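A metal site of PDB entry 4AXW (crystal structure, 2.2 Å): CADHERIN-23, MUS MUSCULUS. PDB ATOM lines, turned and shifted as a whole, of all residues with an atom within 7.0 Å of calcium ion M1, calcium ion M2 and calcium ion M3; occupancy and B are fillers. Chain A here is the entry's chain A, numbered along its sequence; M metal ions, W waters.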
ATOM      1  N   GLU A  22     -37.108   9.923  -9.088  1.00  0.00           N
ATOM      2  CA  GLU A  22     -37.664   9.081  -8.043  1.00  0.00           C
ATOM      3  C   GLU A  22     -38.119   9.874  -6.829  1.00  0.00           C
ATOM      4  O   GLU A  22     -38.815   9.325  -5.985  1.00  0.00           O
ATOM      5  CB  GLU A  22     -36.707   7.961  -7.612  1.00  0.00           C
ATOM      6  CG  GLU A  22     -35.481   8.407  -6.835  1.00  0.00           C
ATOM      7  CD  GLU A  22     -34.639   7.241  -6.308  1.00  0.00           C
ATOM      8  OE1 GLU A  22     -35.250   6.230  -5.914  1.00  0.00           O
ATOM      9  OE2 GLU A  22     -33.385   7.364  -6.229  1.00  0.00           O
ATOM     10  N   LEU A  71     -42.158   6.332  -6.441  1.00  0.00           N
ATOM     11  CA  LEU A  71     -41.265   5.610  -7.303  1.00  0.00           C
ATOM     12  C   LEU A  71     -39.994   5.285  -6.481  1.00  0.00           C
ATOM     13  O   LEU A  71     -39.759   5.919  -5.470  1.00  0.00           O
ATOM     14  CB  LEU A  71     -40.920   6.427  -8.550  1.00  0.00           C
ATOM     15  CG  LEU A  71     -41.969   6.769  -9.619  1.00  0.00           C
ATOM     16  CD1 LEU A  71     -41.400   7.798 -10.582  1.00  0.00           C
ATOM     17  CD2 LEU A  71     -42.471   5.554 -10.423  1.00  0.00           C
ATOM     18  N   ASP A  72     -39.245   4.268  -6.863  1.00  0.00           N
ATOM     19  CA  ASP A  72     -37.951   3.955  -6.214  1.00  0.00           C
ATOM     20  C   ASP A  72     -37.063   3.299  -7.248  1.00  0.00           C
ATOM     21  O   ASP A  72     -37.256   2.142  -7.537  1.00  0.00           O
ATOM     22  CB  ASP A  72     -38.134   3.007  -5.014  1.00  0.00           C
ATOM     23  CG  ASP A  72     -36.785   2.614  -4.341  1.00  0.00           C
ATOM     24  OD1 ASP A  72     -35.733   3.221  -4.654  1.00  0.00           O
ATOM     25  OD2 ASP A  72     -36.769   1.696  -3.488  1.00  0.00           O
ATOM     26  N   ARG A  73     -36.106   4.067  -7.798  1.00  0.00           N
ATOM     27  CA  ARG A  73     -35.219   3.638  -8.886  1.00  0.00           C
ATOM     28  C   ARG A  73     -34.393   2.378  -8.533  1.00  0.00           C
ATOM     29  O   ARG A  73     -34.082   1.578  -9.409  1.00  0.00           O
ATOM     30  CB  ARG A  73     -34.232   4.760  -9.219  1.00  0.00           C
ATOM     31  CG  ARG A  73     -33.407   4.472 -10.527  1.00  0.00           C
ATOM     32  CD  ARG A  73     -32.045   5.145 -10.579  1.00  0.00           C
ATOM     33  NE  ARG A  73     -31.120   4.674  -9.520  1.00  0.00           N
ATOM     34  CZ  ARG A  73     -30.364   3.590  -9.590  1.00  0.00           C
ATOM     35  NH1 ARG A  73     -30.363   2.890 -10.680  1.00  0.00           N
ATOM     36  NH2 ARG A  73     -29.563   3.204  -8.591  1.00  0.00           N
ATOM     37  N   GLU A  74     -34.019   2.242  -7.270  1.00  0.00           N
ATOM     38  CA  GLU A  74     -33.286   1.087  -6.802  1.00  0.00           C
ATOM     39  C   GLU A  74     -34.140  -0.198  -6.820  1.00  0.00           C
ATOM     40  O   GLU A  74     -33.578  -1.306  -6.776  1.00  0.00           O
ATOM     41  CB  GLU A  74     -32.758   1.321  -5.381  1.00  0.00           C
ATOM     42  CG  GLU A  74     -31.553   2.281  -5.291  1.00  0.00           C
ATOM     43  CD  GLU A  74     -31.845   3.776  -5.610  1.00  0.00           C
ATOM     44  OE1 GLU A  74     -32.815   4.379  -5.099  1.00  0.00           O
ATOM     45  OE2 GLU A  74     -31.042   4.400  -6.320  1.00  0.00           O
ATOM     46  N   THR A  75     -35.465  -0.039  -6.859  1.00  0.00           N
ATOM     47  CA  THR A  75     -36.401  -1.159  -6.782  1.00  0.00           C
ATOM     48  C   THR A  75     -36.959  -1.473  -8.152  1.00  0.00           C
ATOM     49  O   THR A  75     -37.117  -2.625  -8.468  1.00  0.00           O
ATOM     50  CB  THR A  75     -37.593  -0.875  -5.829  1.00  0.00           C
ATOM     51  OG1 THR A  75     -37.179  -1.085  -4.468  1.00  0.00           O
ATOM     52  CG2 THR A  75     -38.783  -1.791  -6.141  1.00  0.00           C
ATOM     53  N   GLY A 101     -35.524   8.667 -12.709  1.00  0.00           N
ATOM     54  CA  GLY A 101     -34.312   9.395 -12.353  1.00  0.00           C
ATOM     55  C   GLY A 101     -33.841   9.120 -10.935  1.00  0.00           C
ATOM     56  O   GLY A 101     -34.636   9.027 -10.011  1.00  0.00           O
ATOM     57  N   ASP A 102     -32.532   9.036 -10.758  1.00  0.00           N
ATOM     58  CA  ASP A 102     -31.937   8.839  -9.448  1.00  0.00           C
ATOM     59  C   ASP A 102     -31.872  10.091  -8.636  1.00  0.00           C
ATOM     60  O   ASP A 102     -31.556  11.182  -9.177  1.00  0.00           O
ATOM     61  CB  ASP A 102     -30.529   8.302  -9.592  1.00  0.00           C
ATOM     62  CG  ASP A 102     -30.013   7.679  -8.285  1.00  0.00           C
ATOM     63  OD1 ASP A 102     -30.715   6.787  -7.690  1.00  0.00           O
ATOM     64  OD2 ASP A 102     -28.912   8.107  -7.853  1.00  0.00           O
ATOM     65  N   VAL A 103     -32.092   9.938  -7.326  1.00  0.00           N
ATOM     66  CA  VAL A 103     -31.522  10.839  -6.350  1.00  0.00           C
ATOM     67  C   VAL A 103     -30.698  10.050  -5.309  1.00  0.00           C
ATOM     68  O   VAL A 103     -30.825   8.830  -5.166  1.00  0.00           O
ATOM     69  CB  VAL A 103     -32.602  11.730  -5.644  1.00  0.00           C
ATOM     70  CG1 VAL A 103     -33.550  12.444  -6.680  1.00  0.00           C
ATOM     71  CG2 VAL A 103     -33.419  10.954  -4.617  1.00  0.00           C
ATOM     72  N   ASN A 104     -29.825  10.744  -4.588  1.00  0.00           N
ATOM     73  CA  ASN A 104     -29.074  10.089  -3.541  1.00  0.00           C
ATOM     74  C   ASN A 104     -30.004   9.858  -2.350  1.00  0.00           C
ATOM     75  O   ASN A 104     -30.268  10.781  -1.609  1.00  0.00           O
ATOM     76  CB  ASN A 104     -27.848  10.898  -3.147  1.00  0.00           C
ATOM     77  CG  ASN A 104     -26.964  10.132  -2.193  1.00  0.00           C
ATOM     78  OD1 ASN A 104     -26.657   8.921  -2.420  1.00  0.00           O
ATOM     79  ND2 ASN A 104     -26.574  10.797  -1.089  1.00  0.00           N
ATOM     80  N   ASP A 105     -30.570   8.667  -2.210  1.00  0.00           N
ATOM     81  CA  ASP A 105     -31.423   8.393  -1.044  1.00  0.00           C
ATOM     82  C   ASP A 105     -31.003   7.167  -0.288  1.00  0.00           C
ATOM     83  O   ASP A 105     -31.767   6.698   0.554  1.00  0.00           O
ATOM     84  CB  ASP A 105     -32.908   8.292  -1.409  1.00  0.00           C
ATOM     85  CG  ASP A 105     -33.205   7.344  -2.634  1.00  0.00           C
ATOM     86  OD1 ASP A 105     -32.284   6.778  -3.304  1.00  0.00           O
ATOM     87  OD2 ASP A 105     -34.411   7.245  -2.969  1.00  0.00           O
ATOM     88  N   ASN A 106     -29.816   6.637  -0.546  1.00  0.00           N
ATOM     89  CA  ASN A 106     -29.293   5.570   0.293  1.00  0.00           C
ATOM     90  C   ASN A 106     -28.008   5.918   0.942  1.00  0.00           C
ATOM     91  O   ASN A 106     -27.156   6.570   0.329  1.00  0.00           O
ATOM     92  CB  ASN A 106     -29.115   4.307  -0.523  1.00  0.00           C
ATOM     93  CG  ASN A 106     -30.420   3.755  -1.030  1.00  0.00           C
ATOM     94  OD1 ASN A 106     -30.925   2.811  -0.475  1.00  0.00           O
ATOM     95  ND2 ASN A 106     -31.003   4.397  -2.063  1.00  0.00           N
ATOM     96  N   ALA A 107     -27.831   5.439   2.164  1.00  0.00           N
ATOM     97  CA  ALA A 107     -26.506   5.493   2.798  1.00  0.00           C
ATOM     98  C   ALA A 107     -25.737   4.207   2.489  1.00  0.00           C
ATOM     99  O   ALA A 107     -26.350   3.193   2.164  1.00  0.00           O
ATOM    100  CB  ALA A 107     -26.692   5.666   4.303  1.00  0.00           C
ATOM    101  N   PRO A 108     -24.400   4.220   2.628  1.00  0.00           N
ATOM    102  CA  PRO A 108     -23.635   2.947   2.484  1.00  0.00           C
ATOM    103  C   PRO A 108     -23.961   1.856   3.502  1.00  0.00           C
ATOM    104  O   PRO A 108     -24.396   2.168   4.598  1.00  0.00           O
ATOM    105  CB  PRO A 108     -22.172   3.358   2.618  1.00  0.00           C
ATOM    106  CG  PRO A 108     -22.152   4.838   2.421  1.00  0.00           C
ATOM    107  CD  PRO A 108     -23.500   5.381   2.810  1.00  0.00           C
ATOM    108  N   ASP A 136     -22.986   1.079  -1.851  1.00  0.00           N
ATOM    109  CA  ASP A 136     -24.038   2.105  -1.863  1.00  0.00           C
ATOM    110  C   ASP A 136     -24.677   2.032  -3.242  1.00  0.00           C
ATOM    111  O   ASP A 136     -23.995   2.217  -4.224  1.00  0.00           O
ATOM    112  CB  ASP A 136     -23.432   3.500  -1.601  1.00  0.00           C
ATOM    113  CG  ASP A 136     -24.483   4.586  -1.434  1.00  0.00           C
ATOM    114  OD1 ASP A 136     -25.459   4.606  -2.245  1.00  0.00           O
ATOM    115  OD2 ASP A 136     -24.291   5.482  -0.565  1.00  0.00           O
ATOM    116  N   PRO A 137     -25.980   1.764  -3.333  1.00  0.00           N
ATOM    117  CA  PRO A 137     -26.587   1.491  -4.649  1.00  0.00           C
ATOM    118  C   PRO A 137     -27.052   2.729  -5.462  1.00  0.00           C
ATOM    119  O   PRO A 137     -27.555   2.558  -6.571  1.00  0.00           O
ATOM    120  CB  PRO A 137     -27.813   0.650  -4.288  1.00  0.00           C
ATOM    121  CG  PRO A 137     -28.285   1.334  -3.016  1.00  0.00           C
ATOM    122  CD  PRO A 137     -26.975   1.756  -2.273  1.00  0.00           C
ATOM    123  N   ASP A 138     -26.912   3.936  -4.940  1.00  0.00           N
ATOM    124  CA  ASP A 138     -27.213   5.130  -5.717  1.00  0.00           C
ATOM    125  C   ASP A 138     -26.248   5.304  -6.886  1.00  0.00           C
ATOM    126  O   ASP A 138     -25.209   4.673  -6.911  1.00  0.00           O
ATOM    127  CB  ASP A 138     -27.179   6.359  -4.839  1.00  0.00           C
ATOM    128  CG  ASP A 138     -28.213   6.307  -3.704  1.00  0.00           C
ATOM    129  OD1 ASP A 138     -29.432   6.257  -4.026  1.00  0.00           O
ATOM    130  OD2 ASP A 138     -27.798   6.346  -2.516  1.00  0.00           O
ATOM    131  N   LEU A 139     -26.591   6.143  -7.858  1.00  0.00           N
ATOM    132  CA  LEU A 139     -25.727   6.351  -9.020  1.00  0.00           C
ATOM    133  C   LEU A 139     -24.675   7.397  -8.741  1.00  0.00           C
ATOM    134  O   LEU A 139     -24.951   8.380  -8.027  1.00  0.00           O
ATOM    135  CB  LEU A 139     -26.552   6.848 -10.223  1.00  0.00           C
ATOM    136  CG  LEU A 139     -27.580   5.880 -10.788  1.00  0.00           C
ATOM    137  CD1 LEU A 139     -28.132   6.491 -12.041  1.00  0.00           C
ATOM    138  CD2 LEU A 139     -26.999   4.451 -11.068  1.00  0.00           C
ATOM    139  N   ALA A 141     -21.564   9.929  -7.999  1.00  0.00           N
ATOM    140  CA  ALA A 141     -20.989  10.344  -6.710  1.00  0.00           C
ATOM    141  C   ALA A 141     -21.785   9.832  -5.506  1.00  0.00           C
ATOM    142  O   ALA A 141     -21.232   9.457  -4.474  1.00  0.00           O
ATOM    143  CB  ALA A 141     -20.850  11.841  -6.659  1.00  0.00           C
ATOM    144  N   GLY A 142     -23.095   9.732  -5.661  1.00  0.00           N
ATOM    145  CA  GLY A 142     -23.918   9.176  -4.580  1.00  0.00           C
ATOM    146  C   GLY A 142     -23.711   7.707  -4.278  1.00  0.00           C
ATOM    147  O   GLY A 142     -24.243   7.220  -3.303  1.00  0.00           O
ATOM    148  N   GLY A 143     -22.941   7.021  -5.104  1.00  0.00           N
ATOM    149  CA  GLY A 143     -22.655   5.587  -4.893  1.00  0.00           C
ATOM    150  C   GLY A 143     -21.175   5.296  -4.681  1.00  0.00           C
ATOM    151  O   GLY A 143     -20.783   4.168  -4.581  1.00  0.00           O
ATOM    152  N   SER A 144     -20.346   6.322  -4.596  1.00  0.00           N
ATOM    153  CA  SER A 144     -18.903   6.125  -4.462  1.00  0.00           C
ATOM    154  C   SER A 144     -18.569   6.393  -3.014  1.00  0.00           C
ATOM    155  O   SER A 144     -18.818   7.479  -2.543  1.00  0.00           O
ATOM    156  CB  SER A 144     -18.180   7.124  -5.371  1.00  0.00           C
ATOM    157  OG  SER A 144     -16.771   6.988  -5.272  1.00  0.00           O
ATOM    158  N   THR A 186     -19.056   7.239   3.845  1.00  0.00           N
ATOM    159  CA  THR A 186     -19.943   8.255   3.290  1.00  0.00           C
ATOM    160  C   THR A 186     -19.937   8.134   1.774  1.00  0.00           C
ATOM    161  O   THR A 186     -18.899   7.754   1.158  1.00  0.00           O
ATOM    162  CB  THR A 186     -19.497   9.677   3.681  1.00  0.00           C
ATOM    163  OG1 THR A 186     -20.369  10.669   3.069  1.00  0.00           O
ATOM    164  CG2 THR A 186     -18.039   9.941   3.276  1.00  0.00           C
ATOM    165  N   ASP A 187     -21.077   8.420   1.165  1.00  0.00           N
ATOM    166  CA  ASP A 187     -21.084   8.693  -0.249  1.00  0.00           C
ATOM    167  C   ASP A 187     -20.643  10.145  -0.481  1.00  0.00           C
ATOM    168  O   ASP A 187     -20.353  10.868   0.497  1.00  0.00           O
ATOM    169  CB  ASP A 187     -22.409   8.355  -0.933  1.00  0.00           C
ATOM    170  CG  ASP A 187     -23.560   9.180  -0.452  1.00  0.00           C
ATOM    171  OD1 ASP A 187     -23.356  10.394  -0.221  1.00  0.00           O
ATOM    172  OD2 ASP A 187     -24.697   8.605  -0.361  1.00  0.00           O
ATOM    173  N   GLN A 188     -20.529  10.528  -1.767  1.00  0.00           N
ATOM    174  CA  GLN A 188     -19.926  11.810  -2.167  1.00  0.00           C
ATOM    175  C   GLN A 188     -20.895  12.706  -2.903  1.00  0.00           C
ATOM    176  O   GLN A 188     -20.496  13.580  -3.657  1.00  0.00           O
ATOM    177  CB  GLN A 188     -18.742  11.554  -3.068  1.00  0.00           C
ATOM    178  CG  GLN A 188     -17.565  10.881  -2.353  1.00  0.00           C
ATOM    179  CD  GLN A 188     -16.333  10.757  -3.239  1.00  0.00           C
ATOM    180  OE1 GLN A 188     -15.509  11.691  -3.312  1.00  0.00           O
ATOM    181  NE2 GLN A 188     -16.212   9.619  -3.934  1.00  0.00           N
ATOM    182  N   ASP A 189     -22.181  12.480  -2.711  1.00  0.00           N
ATOM    183  CA  ASP A 189     -23.188  13.339  -3.297  1.00  0.00           C
ATOM    184  C   ASP A 189     -22.910  14.771  -2.871  1.00  0.00           C
ATOM    185  O   ASP A 189     -22.699  15.035  -1.684  1.00  0.00           O
ATOM    186  CB  ASP A 189     -24.558  12.972  -2.801  1.00  0.00           C
ATOM    187  CG  ASP A 189     -25.655  13.692  -3.559  1.00  0.00           C
ATOM    188  OD1 ASP A 189     -25.894  13.381  -4.767  1.00  0.00           O
ATOM    189  OD2 ASP A 189     -26.330  14.519  -2.920  1.00  0.00           O
ATOM    190  N   ARG A 192     -26.519  16.422  -0.767  1.00  0.00           N
ATOM    191  CA  ARG A 192     -26.997  15.611   0.340  1.00  0.00           C
ATOM    192  C   ARG A 192     -26.149  14.334   0.578  1.00  0.00           C
ATOM    193  O   ARG A 192     -26.633  13.215   0.491  1.00  0.00           O
ATOM    194  CB  ARG A 192     -28.483  15.267   0.084  1.00  0.00           C
ATOM    195  CG  ARG A 192     -29.387  16.497  -0.103  1.00  0.00           C
ATOM    196  CD  ARG A 192     -30.848  16.180  -0.359  1.00  0.00           C
ATOM    197  NE  ARG A 192     -31.371  15.380   0.742  1.00  0.00           N
ATOM    198  CZ  ARG A 192     -31.555  14.064   0.718  1.00  0.00           C
ATOM    199  NH1 ARG A 192     -31.362  13.366  -0.404  1.00  0.00           N
ATOM    200  NH2 ARG A 192     -31.920  13.445   1.844  1.00  0.00           N
ATOM    201  N   PRO A 193     -24.880  14.476   0.935  1.00  0.00           N
ATOM    202  CA  PRO A 193     -24.168  13.233   1.282  1.00  0.00           C
ATOM    203  C   PRO A 193     -24.802  12.371   2.415  1.00  0.00           C
ATOM    204  O   PRO A 193     -25.296  12.899   3.416  1.00  0.00           O
ATOM    205  CB  PRO A 193     -22.812  13.726   1.723  1.00  0.00           C
ATOM    206  CG  PRO A 193     -23.066  15.158   2.225  1.00  0.00           C
ATOM    207  CD  PRO A 193     -24.136  15.696   1.313  1.00  0.00           C
ATOM    208  N   LEU A 194     -24.731  11.054   2.286  1.00  0.00           N
ATOM    209  CA  LEU A 194     -25.249  10.194   3.356  1.00  0.00           C
ATOM    210  C   LEU A 194     -24.175   9.258   3.841  1.00  0.00           C
ATOM    211  O   LEU A 194     -23.275   8.828   3.061  1.00  0.00           O
ATOM    212  CB  LEU A 194     -26.464   9.380   2.866  1.00  0.00           C
ATOM    213  CG  LEU A 194     -27.696  10.192   2.408  1.00  0.00           C
ATOM    214  CD1 LEU A 194     -28.684   9.275   1.689  1.00  0.00           C
ATOM    215  CD2 LEU A 194     -28.393  10.890   3.620  1.00  0.00           C
HETATM  216 CA    CA M   1     -34.669   5.060  -3.971  1.00  0.00          CA
HETATM  217 CA    CA M   2     -31.368   6.619  -5.440  1.00  0.00          CA
HETATM  218 CA    CA M   3     -25.812   6.958  -1.483  1.00  0.00          CA
HETATM  219  O   HOH W   1     -36.817   5.418  -2.903  1.00  0.00           O
HETATM  220  O   HOH W   2     -34.123   3.844  -2.108  1.00  0.00           O
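The nearest printed residue that does not touch calcium ion M3 is Ala 107 (4.4 Å).
Of the 29 residues printed, 6 come within 4 Å of calcium ion M2. Along chain A the residues within 4 Å of calcium ion M2 span positions 22 to 138. The nearest printed residue that does not touch calcium ion M2 is Asn 106 (4.1 Å).
Calcium ion M3 is bound by OD2 of Asp 187 (2.3 Å), O of Asn 106 (2.3 Å), OD2 of Asp 136 (2.3 Å), OD2 of Asp 138 (2.3 Å), OD1 of Asn 104 (2.3 Å), O of Gly 142 (2.4 Å) and OD1 of Asp 136 (2.5 Å). Calcium ion M3 has seven donor atoms within binding distance.
Of the 29 residues printed, 4 come within 4 Å of calcium ion M1. The nearest printed residue that does not touch calcium ion M1 is Asn 106 (4.2 Å).
Calcium ion M1 is bound by OD1 of Asp 72 (2.2 Å). OE1 of Glu 74 is bound to calcium ion M1 (2.3 Å). Water W2 binds calcium ion M1 (2.3 Å). OE1 of Glu 22 binds calcium ion M1. The side-chain carboxylate (OD2) of Asp 105 binds calcium ion M1 (2.4 Å). Water W1 binds calcium ion M1 (2.4 Å). Slightly farther from calcium ion M1 lies OD1 of Asp 105 (3.0 Å).
Calcium ion M2 is bound by OE2 of Glu 22 (2.3 Å), O of Val 103 (2.3 Å), OD1 of Asp 105 (2.3 Å), OD1 of Asp 102 (2.3 Å), OE2 of Glu 74 (2.4 Å), OD1 of Asp 138 (2.4 Å) and OE1 of Glu 74 (2.7 Å).
OD2 of Asp 102 is in hydrogen-bond range of N of Leu 139, 3.0 Å away. The backbone NH (N) of Asp 187 lies within hydrogen-bond range of the backbone carbonyl oxygen (O) of Leu 194, 2.9 Å away. The side-chain amide nitrogen (ND2) of Asn 104 sits at hydrogen-bond distance from the backbone carbonyl oxygen (O) of Arg 192 (2.9 Å). The backbone carbonyl oxygen (O) of Gly 101 sits at hydrogen-bond distance from the backbone NH (N) of Glu 22, at 2.8 Å. The side-chain carboxylate of Asp 102 sits close to the guanidinium group of Arg 73 (2.8 Å). The side-chain carboxylate (OD1) of Asp 187 is in hydrogen-bond range of the backbone NH (N) of Asp 189, 3.5 Å away. OD1 of Asp 105 lies close to ND2 of Asn 106. The side-chain hydroxyl (OG1) of Thr 75 is in hydrogen-bond range of the side-chain carboxylate (OD2) of Asp 72 (3.0 Å).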
